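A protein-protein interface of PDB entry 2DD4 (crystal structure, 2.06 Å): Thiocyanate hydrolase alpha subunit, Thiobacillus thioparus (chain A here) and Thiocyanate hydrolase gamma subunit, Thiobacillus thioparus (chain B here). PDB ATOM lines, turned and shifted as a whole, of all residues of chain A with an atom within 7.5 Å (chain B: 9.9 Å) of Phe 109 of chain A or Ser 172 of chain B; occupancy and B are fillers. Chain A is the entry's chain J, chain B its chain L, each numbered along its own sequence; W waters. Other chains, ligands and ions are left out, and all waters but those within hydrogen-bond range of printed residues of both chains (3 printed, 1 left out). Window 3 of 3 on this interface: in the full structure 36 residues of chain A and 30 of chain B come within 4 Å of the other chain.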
ATOM      1  N   GLN A  98       1.018  -4.720   8.779  1.00  0.00           N
ATOM      2  CA  GLN A  98       2.069  -5.448   8.069  1.00  0.00           C
ATOM      3  C   GLN A  98       1.688  -5.805   6.630  1.00  0.00           C
ATOM      4  O   GLN A  98       2.529  -5.757   5.730  1.00  0.00           O
ATOM      5  CB  GLN A  98       2.460  -6.711   8.844  1.00  0.00           C
ATOM      6  CG  GLN A  98       3.268  -6.434  10.111  1.00  0.00           C
ATOM      7  CD  GLN A  98       4.707  -6.032   9.818  1.00  0.00           C
ATOM      8  OE1 GLN A  98       4.968  -5.148   8.998  1.00  0.00           O
ATOM      9  NE2 GLN A  98       5.651  -6.678  10.495  1.00  0.00           N
ATOM     10  N   LYS A  99       0.422  -6.149   6.408  1.00  0.00           N
ATOM     11  CA  LYS A  99      -0.030  -6.504   5.066  1.00  0.00           C
ATOM     12  C   LYS A  99       0.080  -5.334   4.087  1.00  0.00           C
ATOM     13  O   LYS A  99       0.109  -5.541   2.876  1.00  0.00           O
ATOM     14  CB  LYS A  99      -1.472  -7.011   5.105  1.00  0.00           C
ATOM     15  CG  LYS A  99      -2.499  -5.940   5.444  1.00  0.00           C
ATOM     16  CD  LYS A  99      -3.850  -6.558   5.789  1.00  0.00           C
ATOM     17  CE  LYS A  99      -4.379  -7.442   4.665  1.00  0.00           C
ATOM     18  NZ  LYS A  99      -5.657  -8.121   5.039  1.00  0.00           N
ATOM     19  N   TYR A 105       2.628 -11.007   3.374  1.00  0.00           N
ATOM     20  CA  TYR A 105       2.197 -11.204   4.754  1.00  0.00           C
ATOM     21  C   TYR A 105       0.912 -12.021   4.806  1.00  0.00           C
ATOM     22  O   TYR A 105      -0.038 -11.757   4.072  1.00  0.00           O
ATOM     23  CB  TYR A 105       2.001  -9.868   5.480  1.00  0.00           C
ATOM     24  CG  TYR A 105       2.471  -9.934   6.918  1.00  0.00           C
ATOM     25  CD1 TYR A 105       3.833  -9.927   7.220  1.00  0.00           C
ATOM     26  CD2 TYR A 105       1.563 -10.073   7.971  1.00  0.00           C
ATOM     27  CE1 TYR A 105       4.287 -10.059   8.531  1.00  0.00           C
ATOM     28  CE2 TYR A 105       2.008 -10.210   9.293  1.00  0.00           C
ATOM     29  CZ  TYR A 105       3.373 -10.203   9.561  1.00  0.00           C
ATOM     30  OH  TYR A 105       3.831 -10.346  10.852  1.00  0.00           O
ATOM     31  N   SER A 106       0.892 -13.015   5.685  1.00  0.00           N
ATOM     32  CA  SER A 106      -0.252 -13.909   5.823  1.00  0.00           C
ATOM     33  C   SER A 106      -1.464 -13.335   6.550  1.00  0.00           C
ATOM     34  O   SER A 106      -1.329 -12.664   7.573  1.00  0.00           O
ATOM     35  CB  SER A 106       0.191 -15.193   6.527  1.00  0.00           C
ATOM     36  OG  SER A 106      -0.923 -16.011   6.846  1.00  0.00           O
ATOM     37  N   ASP A 107      -2.650 -13.617   6.018  1.00  0.00           N
ATOM     38  CA  ASP A 107      -3.885 -13.154   6.637  1.00  0.00           C
ATOM     39  C   ASP A 107      -4.067 -13.848   7.982  1.00  0.00           C
ATOM     40  O   ASP A 107      -4.874 -13.419   8.799  1.00  0.00           O
ATOM     41  CB  ASP A 107      -5.098 -13.458   5.754  1.00  0.00           C
ATOM     42  CG  ASP A 107      -5.115 -12.644   4.482  1.00  0.00           C
ATOM     43  OD1 ASP A 107      -4.582 -11.513   4.485  1.00  0.00           O
ATOM     44  OD2 ASP A 107      -5.680 -13.131   3.481  1.00  0.00           O
ATOM     45  N   THR A 108      -3.323 -14.929   8.204  1.00  0.00           N
ATOM     46  CA  THR A 108      -3.410 -15.657   9.467  1.00  0.00           C
ATOM     47  C   THR A 108      -2.966 -14.735  10.600  1.00  0.00           C
ATOM     48  O   THR A 108      -3.464 -14.818  11.719  1.00  0.00           O
ATOM     49  CB  THR A 108      -2.507 -16.918   9.466  1.00  0.00           C
ATOM     50  OG1 THR A 108      -3.028 -17.885   8.545  1.00  0.00           O
ATOM     51  CG2 THR A 108      -2.455 -17.543  10.857  1.00  0.00           C
ATOM     52  N   PHE A 109      -2.021 -13.854  10.299  1.00  0.00           N
ATOM     53  CA  PHE A 109      -1.508 -12.909  11.287  1.00  0.00           C
ATOM     54  C   PHE A 109      -2.009 -11.516  10.902  1.00  0.00           C
ATOM     55  O   PHE A 109      -1.238 -10.562  10.780  1.00  0.00           O
ATOM     56  CB  PHE A 109       0.018 -12.966  11.288  1.00  0.00           C
ATOM     57  CG  PHE A 109       0.565 -14.361  11.443  1.00  0.00           C
ATOM     58  CD1 PHE A 109       0.309 -15.098  12.598  1.00  0.00           C
ATOM     59  CD2 PHE A 109       1.321 -14.943  10.432  1.00  0.00           C
ATOM     60  CE1 PHE A 109       0.800 -16.396  12.740  1.00  0.00           C
ATOM     61  CE2 PHE A 109       1.818 -16.242  10.564  1.00  0.00           C
ATOM     62  CZ  PHE A 109       1.555 -16.969  11.720  1.00  0.00           C
ATOM     63  N   ALA A 110      -3.323 -11.426  10.729  1.00  0.00           N
ATOM     64  CA  ALA A 110      -4.006 -10.203  10.315  1.00  0.00           C
ATOM     65  C   ALA A 110      -3.841  -8.957  11.178  1.00  0.00           C
ATOM     66  O   ALA A 110      -4.022  -7.844  10.685  1.00  0.00           O
ATOM     67  CB  ALA A 110      -5.491 -10.496  10.139  1.00  0.00           C
ATOM     68  N   ASN A 111      -3.496  -9.121  12.448  1.00  0.00           N
ATOM     69  CA  ASN A 111      -3.369  -7.963  13.324  1.00  0.00           C
ATOM     70  C   ASN A 111      -1.958  -7.418  13.532  1.00  0.00           C
ATOM     71  O   ASN A 111      -1.784  -6.408  14.215  1.00  0.00           O
ATOM     72  CB  ASN A 111      -4.000  -8.280  14.680  1.00  0.00           C
ATOM     73  CG  ASN A 111      -5.446  -8.725  14.554  1.00  0.00           C
ATOM     74  OD1 ASN A 111      -6.244  -8.082  13.872  1.00  0.00           O
ATOM     75  ND2 ASN A 111      -5.790  -9.825  15.213  1.00  0.00           N
ATOM     76  N   ASP A 112      -0.959  -8.072  12.951  1.00  0.00           N
ATOM     77  CA  ASP A 112       0.419  -7.625  13.110  1.00  0.00           C
ATOM     78  C   ASP A 112       0.638  -6.233  12.528  1.00  0.00           C
ATOM     79  O   ASP A 112       0.069  -5.878  11.493  1.00  0.00           O
ATOM     80  CB  ASP A 112       1.382  -8.628  12.473  1.00  0.00           C
ATOM     81  CG  ASP A 112       1.452  -9.933  13.242  1.00  0.00           C
ATOM     82  OD1 ASP A 112       0.771 -10.053  14.286  1.00  0.00           O
ATOM     83  OD2 ASP A 112       2.191 -10.839  12.810  1.00  0.00           O
ATOM     84  N   THR A 113       1.477  -5.450  13.197  1.00  0.00           N
ATOM     85  CA  THR A 113       1.744  -4.086  12.769  1.00  0.00           C
ATOM     86  C   THR A 113       3.208  -3.700  12.926  1.00  0.00           C
ATOM     87  O   THR A 113       4.018  -4.463  13.458  1.00  0.00           O
ATOM     88  CB  THR A 113       0.917  -3.094  13.596  1.00  0.00           C
ATOM     89  OG1 THR A 113       1.231  -3.279  14.981  1.00  0.00           O
ATOM     90  CG2 THR A 113      -0.583  -3.318  13.387  1.00  0.00           C
ATOM     91  N   PRO B 120      -2.567  -8.938  26.670  1.00  0.00           N
ATOM     92  CA  PRO B 120      -3.019 -10.238  26.164  1.00  0.00           C
ATOM     93  C   PRO B 120      -3.222 -10.237  24.642  1.00  0.00           C
ATOM     94  O   PRO B 120      -3.238 -11.291  24.010  1.00  0.00           O
ATOM     95  CB  PRO B 120      -4.332 -10.460  26.916  1.00  0.00           C
ATOM     96  CG  PRO B 120      -4.076  -9.792  28.231  1.00  0.00           C
ATOM     97  CD  PRO B 120      -3.399  -8.502  27.809  1.00  0.00           C
ATOM     98  N   THR B 121      -3.368  -9.051  24.059  1.00  0.00           N
ATOM     99  CA  THR B 121      -3.589  -8.925  22.621  1.00  0.00           C
ATOM    100  C   THR B 121      -2.505  -8.135  21.883  1.00  0.00           C
ATOM    101  O   THR B 121      -2.648  -7.851  20.692  1.00  0.00           O
ATOM    102  CB  THR B 121      -4.927  -8.233  22.347  1.00  0.00           C
ATOM    103  OG1 THR B 121      -4.893  -6.913  22.904  1.00  0.00           O
ATOM    104  CG2 THR B 121      -6.076  -9.012  22.984  1.00  0.00           C
ATOM    105  N   LEU B 122      -1.427  -7.784  22.580  1.00  0.00           N
ATOM    106  CA  LEU B 122      -0.344  -7.009  21.972  1.00  0.00           C
ATOM    107  C   LEU B 122       1.028  -7.408  22.513  1.00  0.00           C
ATOM    108  O   LEU B 122       1.237  -7.461  23.724  1.00  0.00           O
ATOM    109  CB  LEU B 122      -0.583  -5.513  22.219  1.00  0.00           C
ATOM    110  CG  LEU B 122       0.467  -4.494  21.761  1.00  0.00           C
ATOM    111  CD1 LEU B 122       0.611  -4.534  20.237  1.00  0.00           C
ATOM    112  CD2 LEU B 122       0.044  -3.099  22.219  1.00  0.00           C
ATOM    113  N   ARG B 157      10.066  -7.482   8.645  1.00  0.00           N
ATOM    114  CA  ARG B 157       9.282  -8.198   7.643  1.00  0.00           C
ATOM    115  C   ARG B 157       8.788  -9.592   8.031  1.00  0.00           C
ATOM    116  O   ARG B 157       7.684  -9.989   7.654  1.00  0.00           O
ATOM    117  CB  ARG B 157      10.092  -8.281   6.347  1.00  0.00           C
ATOM    118  CG  ARG B 157       9.320  -8.801   5.158  1.00  0.00           C
ATOM    119  CD  ARG B 157      10.072  -8.536   3.853  1.00  0.00           C
ATOM    120  NE  ARG B 157       9.187  -8.734   2.711  1.00  0.00           N
ATOM    121  CZ  ARG B 157       9.428  -8.296   1.481  1.00  0.00           C
ATOM    122  NH1 ARG B 157      10.544  -7.627   1.214  1.00  0.00           N
ATOM    123  NH2 ARG B 157       8.530  -8.504   0.525  1.00  0.00           N
ATOM    124  N   TRP B 158       9.610 -10.334   8.762  1.00  0.00           N
ATOM    125  CA  TRP B 158       9.256 -11.686   9.189  1.00  0.00           C
ATOM    126  C   TRP B 158       9.432 -11.800  10.705  1.00  0.00           C
ATOM    127  O   TRP B 158      10.178 -12.649  11.187  1.00  0.00           O
ATOM    128  CB  TRP B 158      10.165 -12.703   8.485  1.00  0.00           C
ATOM    129  CG  TRP B 158      10.088 -12.666   6.981  1.00  0.00           C
ATOM    130  CD1 TRP B 158       9.110 -13.208   6.192  1.00  0.00           C
ATOM    131  CD2 TRP B 158      11.032 -12.058   6.085  1.00  0.00           C
ATOM    132  NE1 TRP B 158       9.388 -12.978   4.864  1.00  0.00           N
ATOM    133  CE2 TRP B 158      10.561 -12.275   4.769  1.00  0.00           C
ATOM    134  CE3 TRP B 158      12.229 -11.352   6.267  1.00  0.00           C
ATOM    135  CZ2 TRP B 158      11.246 -11.811   3.638  1.00  0.00           C
ATOM    136  CZ3 TRP B 158      12.915 -10.887   5.135  1.00  0.00           C
ATOM    137  CH2 TRP B 158      12.418 -11.122   3.841  1.00  0.00           C
ATOM    138  N   PRO B 159       8.742 -10.944  11.475  1.00  0.00           N
ATOM    139  CA  PRO B 159       8.857 -10.979  12.937  1.00  0.00           C
ATOM    140  C   PRO B 159       8.465 -12.305  13.580  1.00  0.00           C
ATOM    141  O   PRO B 159       9.127 -12.764  14.504  1.00  0.00           O
ATOM    142  CB  PRO B 159       7.974  -9.813  13.380  1.00  0.00           C
ATOM    143  CG  PRO B 159       6.927  -9.759  12.305  1.00  0.00           C
ATOM    144  CD  PRO B 159       7.733  -9.954  11.050  1.00  0.00           C
ATOM    145  N   ARG B 160       7.389 -12.916  13.090  1.00  0.00           N
ATOM    146  CA  ARG B 160       6.923 -14.201  13.611  1.00  0.00           C
ATOM    147  C   ARG B 160       8.025 -15.252  13.451  1.00  0.00           C
ATOM    148  O   ARG B 160       8.338 -15.995  14.382  1.00  0.00           O
ATOM    149  CB  ARG B 160       5.687 -14.663  12.837  1.00  0.00           C
ATOM    150  CG  ARG B 160       4.463 -13.772  12.988  1.00  0.00           C
ATOM    151  CD  ARG B 160       3.613 -14.217  14.147  1.00  0.00           C
ATOM    152  NE  ARG B 160       2.490 -13.318  14.398  1.00  0.00           N
ATOM    153  CZ  ARG B 160       1.566 -13.542  15.324  1.00  0.00           C
ATOM    154  NH1 ARG B 160       1.638 -14.636  16.071  1.00  0.00           N
ATOM    155  NH2 ARG B 160       0.581 -12.670  15.517  1.00  0.00           N
ATOM    156  N   GLN B 161       8.609 -15.302  12.258  1.00  0.00           N
ATOM    157  CA  GLN B 161       9.661 -16.266  11.965  1.00  0.00           C
ATOM    158  C   GLN B 161      10.932 -16.013  12.774  1.00  0.00           C
ATOM    159  O   GLN B 161      11.505 -16.948  13.345  1.00  0.00           O
ATOM    160  CB  GLN B 161       9.974 -16.260  10.462  1.00  0.00           C
ATOM    161  CG  GLN B 161       8.808 -16.729   9.591  1.00  0.00           C
ATOM    162  CD  GLN B 161       7.796 -15.630   9.276  1.00  0.00           C
ATOM    163  OE1 GLN B 161       7.881 -14.511   9.785  1.00  0.00           O
ATOM    164  NE2 GLN B 161       6.831 -15.953   8.426  1.00  0.00           N
ATOM    165  N   ALA B 164      10.391 -16.888  16.381  1.00  0.00           N
ATOM    166  CA  ALA B 164      10.350 -18.338  16.556  1.00  0.00           C
ATOM    167  C   ALA B 164      11.775 -18.872  16.683  1.00  0.00           C
ATOM    168  O   ALA B 164      12.042 -19.781  17.470  1.00  0.00           O
ATOM    169  CB  ALA B 164       9.645 -18.994  15.375  1.00  0.00           C
ATOM    170  N   LEU B 168      10.405 -17.857  20.647  1.00  0.00           N
ATOM    171  CA  LEU B 168       9.194 -17.185  21.098  1.00  0.00           C
ATOM    172  C   LEU B 168       8.085 -17.247  20.055  1.00  0.00           C
ATOM    173  O   LEU B 168       8.287 -16.909  18.887  1.00  0.00           O
ATOM    174  CB  LEU B 168       9.488 -15.721  21.447  1.00  0.00           C
ATOM    175  CG  LEU B 168       8.279 -14.866  21.845  1.00  0.00           C
ATOM    176  CD1 LEU B 168       7.605 -15.456  23.077  1.00  0.00           C
ATOM    177  CD2 LEU B 168       8.730 -13.438  22.117  1.00  0.00           C
ATOM    178  N   GLN B 169       6.909 -17.683  20.490  1.00  0.00           N
ATOM    179  CA  GLN B 169       5.755 -17.783  19.611  1.00  0.00           C
ATOM    180  C   GLN B 169       4.520 -17.257  20.329  1.00  0.00           C
ATOM    181  O   GLN B 169       4.344 -17.489  21.524  1.00  0.00           O
ATOM    182  CB  GLN B 169       5.540 -19.241  19.199  1.00  0.00           C
ATOM    183  CG  GLN B 169       4.282 -19.489  18.387  1.00  0.00           C
ATOM    184  CD  GLN B 169       4.223 -20.901  17.825  1.00  0.00           C
ATOM    185  OE1 GLN B 169       4.936 -21.239  16.875  1.00  0.00           O
ATOM    186  NE2 GLN B 169       3.375 -21.734  18.417  1.00  0.00           N
ATOM    187  N   LEU B 170       3.676 -16.531  19.602  1.00  0.00           N
ATOM    188  CA  LEU B 170       2.449 -15.995  20.174  1.00  0.00           C
ATOM    189  C   LEU B 170       1.250 -16.382  19.325  1.00  0.00           C
ATOM    190  O   LEU B 170       1.391 -16.684  18.138  1.00  0.00           O
ATOM    191  CB  LEU B 170       2.528 -14.470  20.293  1.00  0.00           C
ATOM    192  CG  LEU B 170       3.474 -14.006  21.404  1.00  0.00           C
ATOM    193  CD1 LEU B 170       4.616 -13.211  20.812  1.00  0.00           C
ATOM    194  CD2 LEU B 170       2.697 -13.188  22.419  1.00  0.00           C
ATOM    195  N   PRO B 171       0.052 -16.398  19.929  1.00  0.00           N
ATOM    196  CA  PRO B 171      -1.167 -16.751  19.198  1.00  0.00           C
ATOM    197  C   PRO B 171      -1.244 -15.944  17.904  1.00  0.00           C
ATOM    198  O   PRO B 171      -0.824 -14.789  17.863  1.00  0.00           O
ATOM    199  CB  PRO B 171      -2.270 -16.383  20.183  1.00  0.00           C
ATOM    200  CG  PRO B 171      -1.634 -16.699  21.507  1.00  0.00           C
ATOM    201  CD  PRO B 171      -0.248 -16.109  21.344  1.00  0.00           C
ATOM    202  N   SER B 172      -1.780 -16.552  16.854  1.00  0.00           N
ATOM    203  CA  SER B 172      -1.884 -15.884  15.565  1.00  0.00           C
ATOM    204  C   SER B 172      -2.764 -14.637  15.604  1.00  0.00           C
ATOM    205  O   SER B 172      -2.570 -13.718  14.809  1.00  0.00           O
ATOM    206  CB  SER B 172      -2.411 -16.861  14.508  1.00  0.00           C
ATOM    207  OG  SER B 172      -3.716 -17.298  14.835  1.00  0.00           O
ATOM    208  N   GLU B 173      -3.724 -14.598  16.524  1.00  0.00           N
ATOM    209  CA  GLU B 173      -4.610 -13.442  16.633  1.00  0.00           C
ATOM    210  C   GLU B 173      -4.000 -12.291  17.434  1.00  0.00           C
ATOM    211  O   GLU B 173      -4.442 -11.150  17.318  1.00  0.00           O
ATOM    212  CB  GLU B 173      -5.961 -13.841  17.241  1.00  0.00           C
ATOM    213  CG  GLU B 173      -5.887 -14.825  18.398  1.00  0.00           C
ATOM    214  CD  GLU B 173      -5.542 -16.232  17.941  1.00  0.00           C
ATOM    215  OE1 GLU B 173      -6.261 -16.770  17.069  1.00  0.00           O
ATOM    216  OE2 GLU B 173      -4.557 -16.801  18.453  1.00  0.00           O
ATOM    217  N   VAL B 174      -2.991 -12.589  18.246  1.00  0.00           N
ATOM    218  CA  VAL B 174      -2.330 -11.549  19.030  1.00  0.00           C
ATOM    219  C   VAL B 174      -1.611 -10.610  18.067  1.00  0.00           C
ATOM    220  O   VAL B 174      -1.038 -11.052  17.071  1.00  0.00           O
ATOM    221  CB  VAL B 174      -1.285 -12.145  20.005  1.00  0.00           C
ATOM    222  CG1 VAL B 174      -0.395 -11.038  20.563  1.00  0.00           C
ATOM    223  CG2 VAL B 174      -1.989 -12.866  21.142  1.00  0.00           C
ATOM    224  N   GLN B 175      -1.651  -9.315  18.360  1.00  0.00           N
ATOM    225  CA  GLN B 175      -0.981  -8.346  17.510  1.00  0.00           C
ATOM    226  C   GLN B 175       0.496  -8.261  17.848  1.00  0.00           C
ATOM    227  O   GLN B 175       0.867  -7.872  18.956  1.00  0.00           O
ATOM    228  CB  GLN B 175      -1.597  -6.951  17.673  1.00  0.00           C
ATOM    229  CG  GLN B 175      -0.818  -5.844  16.952  1.00  0.00           C
ATOM    230  CD  GLN B 175      -1.378  -4.453  17.218  1.00  0.00           C
ATOM    231  OE1 GLN B 175      -2.413  -4.302  17.870  1.00  0.00           O
ATOM    232  NE2 GLN B 175      -0.697  -3.433  16.714  1.00  0.00           N
ATOM    233  N   ILE B 176       1.347  -8.656  16.911  1.00  0.00           N
ATOM    234  CA  ILE B 176       2.773  -8.527  17.150  1.00  0.00           C
ATOM    235  C   ILE B 176       3.132  -7.186  16.528  1.00  0.00           C
ATOM    236  O   ILE B 176       2.858  -6.947  15.352  1.00  0.00           O
ATOM    237  CB  ILE B 176       3.588  -9.655  16.482  1.00  0.00           C
ATOM    238  CG1 ILE B 176       3.441 -10.941  17.302  1.00  0.00           C
ATOM    239  CG2 ILE B 176       5.064  -9.243  16.365  1.00  0.00           C
ATOM    240  CD1 ILE B 176       4.275 -12.094  16.800  1.00  0.00           C
ATOM    241  N   ARG B 177       3.702  -6.293  17.325  1.00  0.00           N
ATOM    242  CA  ARG B 177       4.085  -4.992  16.805  1.00  0.00           C
ATOM    243  C   ARG B 177       5.587  -4.810  16.847  1.00  0.00           C
ATOM    244  O   ARG B 177       6.211  -4.907  17.904  1.00  0.00           O
ATOM    245  CB  ARG B 177       3.418  -3.853  17.590  1.00  0.00           C
ATOM    246  CG  ARG B 177       3.933  -2.472  17.172  1.00  0.00           C
ATOM    247  CD  ARG B 177       3.143  -1.328  17.791  1.00  0.00           C
ATOM    248  NE  ARG B 177       1.730  -1.383  17.428  1.00  0.00           N
ATOM    249  CZ  ARG B 177       0.837  -0.457  17.759  1.00  0.00           C
ATOM    250  NH1 ARG B 177       1.210   0.608  18.459  1.00  0.00           N
ATOM    251  NH2 ARG B 177      -0.436  -0.613  17.418  1.00  0.00           N
HETATM  252  O   HOH W   1       5.786 -12.366  10.663  1.00  0.00           O
HETATM  253  O   HOH W   2       4.480  -7.180  13.285  1.00  0.00           O
HETATM  254  O   HOH W   3      -5.433 -16.130  13.091  1.00  0.00           O
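Water W2 lies within hydrogen-bond range of the backbone carbonyl oxygen of Ile 176 of chain B (2.6 Å), the backbone carbonyl oxygen of Thr 113 of chain A (2.8 Å) and the side-chain amide nitrogen of Gln 98 of chain A (3.1 Å).
Water W3 bridges OG of Ser 172 of chain B and O of Thr 108 of chain A.
Water W1 lies within hydrogen-bond range of the side-chain hydroxyl of Tyr 105 of chain A, the backbone NH of Arg 160 of chain B and the side-chain amide oxygen of Gln 161 of chain B.
Printed residues of chain B that touch a printed residue of chain A: Arg 157, Pro 159, Arg 160, Ser 172, Glu 173, Val 174, Gln 175, Ile 176 and Arg 177.
Of the 11 printed residues of chain A, 7 touch a printed residue of chain B.
Hydrophobic or aromatic side chains of chain A that line the printed part of chain B: Tyr 105 and Phe 109.
Among the printed residues, merely in contact across the chains: Asn 111 of chain A with Gln 175 of chain B, Phe 109 of chain A with Arg 160 of chain B, Tyr 105 of chain A with Pro 159 of chain B, Tyr 105 of chain A with Arg 157 of chain B, Phe 109 of chain A with Ser 172 of chain B, Gln 98 of chain A with Pro 159 of chain B and Asp 112 of chain A with Gln 175 of chain B.
The backbone carbonyl oxygen of Val 174 of chain B sits close to the side-chain carboxylate of Asp 112 of chain A (3.5 Å).
The side-chain hydroxyl (OG1) of Thr 113 of chain A lies within hydrogen-bond range of the guanidinium group (NE) of Arg 177 of chain B (3.1 Å).
NH2 of Arg 160 of chain B lies within salt-bridge range of OD1 of Asp 112 of chain A (2.9 Å).
The backbone carbonyl oxygen (O) of Ser 172 of chain B sits close to the backbone carbonyl oxygen (O) of Thr 108 of chain A, 3.4 Å away.
The backbone carbonyl oxygen (O) of Ile 176 of chain B lies within hydrogen-bond range of the backbone NH (N) of Thr 113 of chain A (3.0 Å).
OG1 of Thr 113 of chain A sits at hydrogen-bond distance from NE2 of Gln 175 of chain B (2.6 Å).
O of Glu 173 of chain B is in hydrogen-bond range of ND2 of Asn 111 of chain A.
The side-chain carboxylate of Asp 112 of chain A sits at hydrogen-bond distance from the backbone NH of Ile 176 of chain B (3.0 Å).
Printed residues of chain B within 4 Å of Gln 98 of chain A: Pro 159 (3.8 Å).
Asp 107 of chain A touches none of the printed residues of chain B.
Thr 108 of chain A touches just one residue of chain B: Ser 172 (3.4 Å).
Phe 109 of chain A touches two residues of chain B.
No residue of chain B comes within 4 Å of Ala 110 of chain A.
Printed residues of chain A within 4 Å of Arg 157 of chain B: Tyr 105.
Ala 164 of chain B touches none of the printed residues of chain A.
The nearest residue of chain B that does not touch Phe 109 of chain A is Pro 171 of chain B (5.4 Å).
The nearest printed residue of chain A that does not touch Arg 160 of chain B is Tyr 105 of chain A (4.1 Å).
The side-chain carboxylate (OD2) of Asp 112 of chain A is in hydrogen-bond range of the side-chain hydroxyl (OH) of Tyr 105 of chain A, 2.6 Å away.
The guanidinium group (NH2) of Arg 177 of chain B lies close to the side-chain amide nitrogen (NE2) of Gln 175 of chain B, at 2.9 Å.
OG of Ser 106 of chain A sits close to N of Thr 108 of chain A, at 3.0 Å.
O of Ser 172 of chain B sits at hydrogen-bond distance from NH2 of Arg 160 of chain B (3.4 Å).
The guanidinium group of Arg 160 of chain B sits at hydrogen-bond distance from the backbone carbonyl oxygen of Leu 170 of chain B, at 2.9 Å.
The backbone NH of Gln 98 of chain A lies within hydrogen-bond range of the backbone carbonyl oxygen of Asp 112 of chain A, 3.1 Å away.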
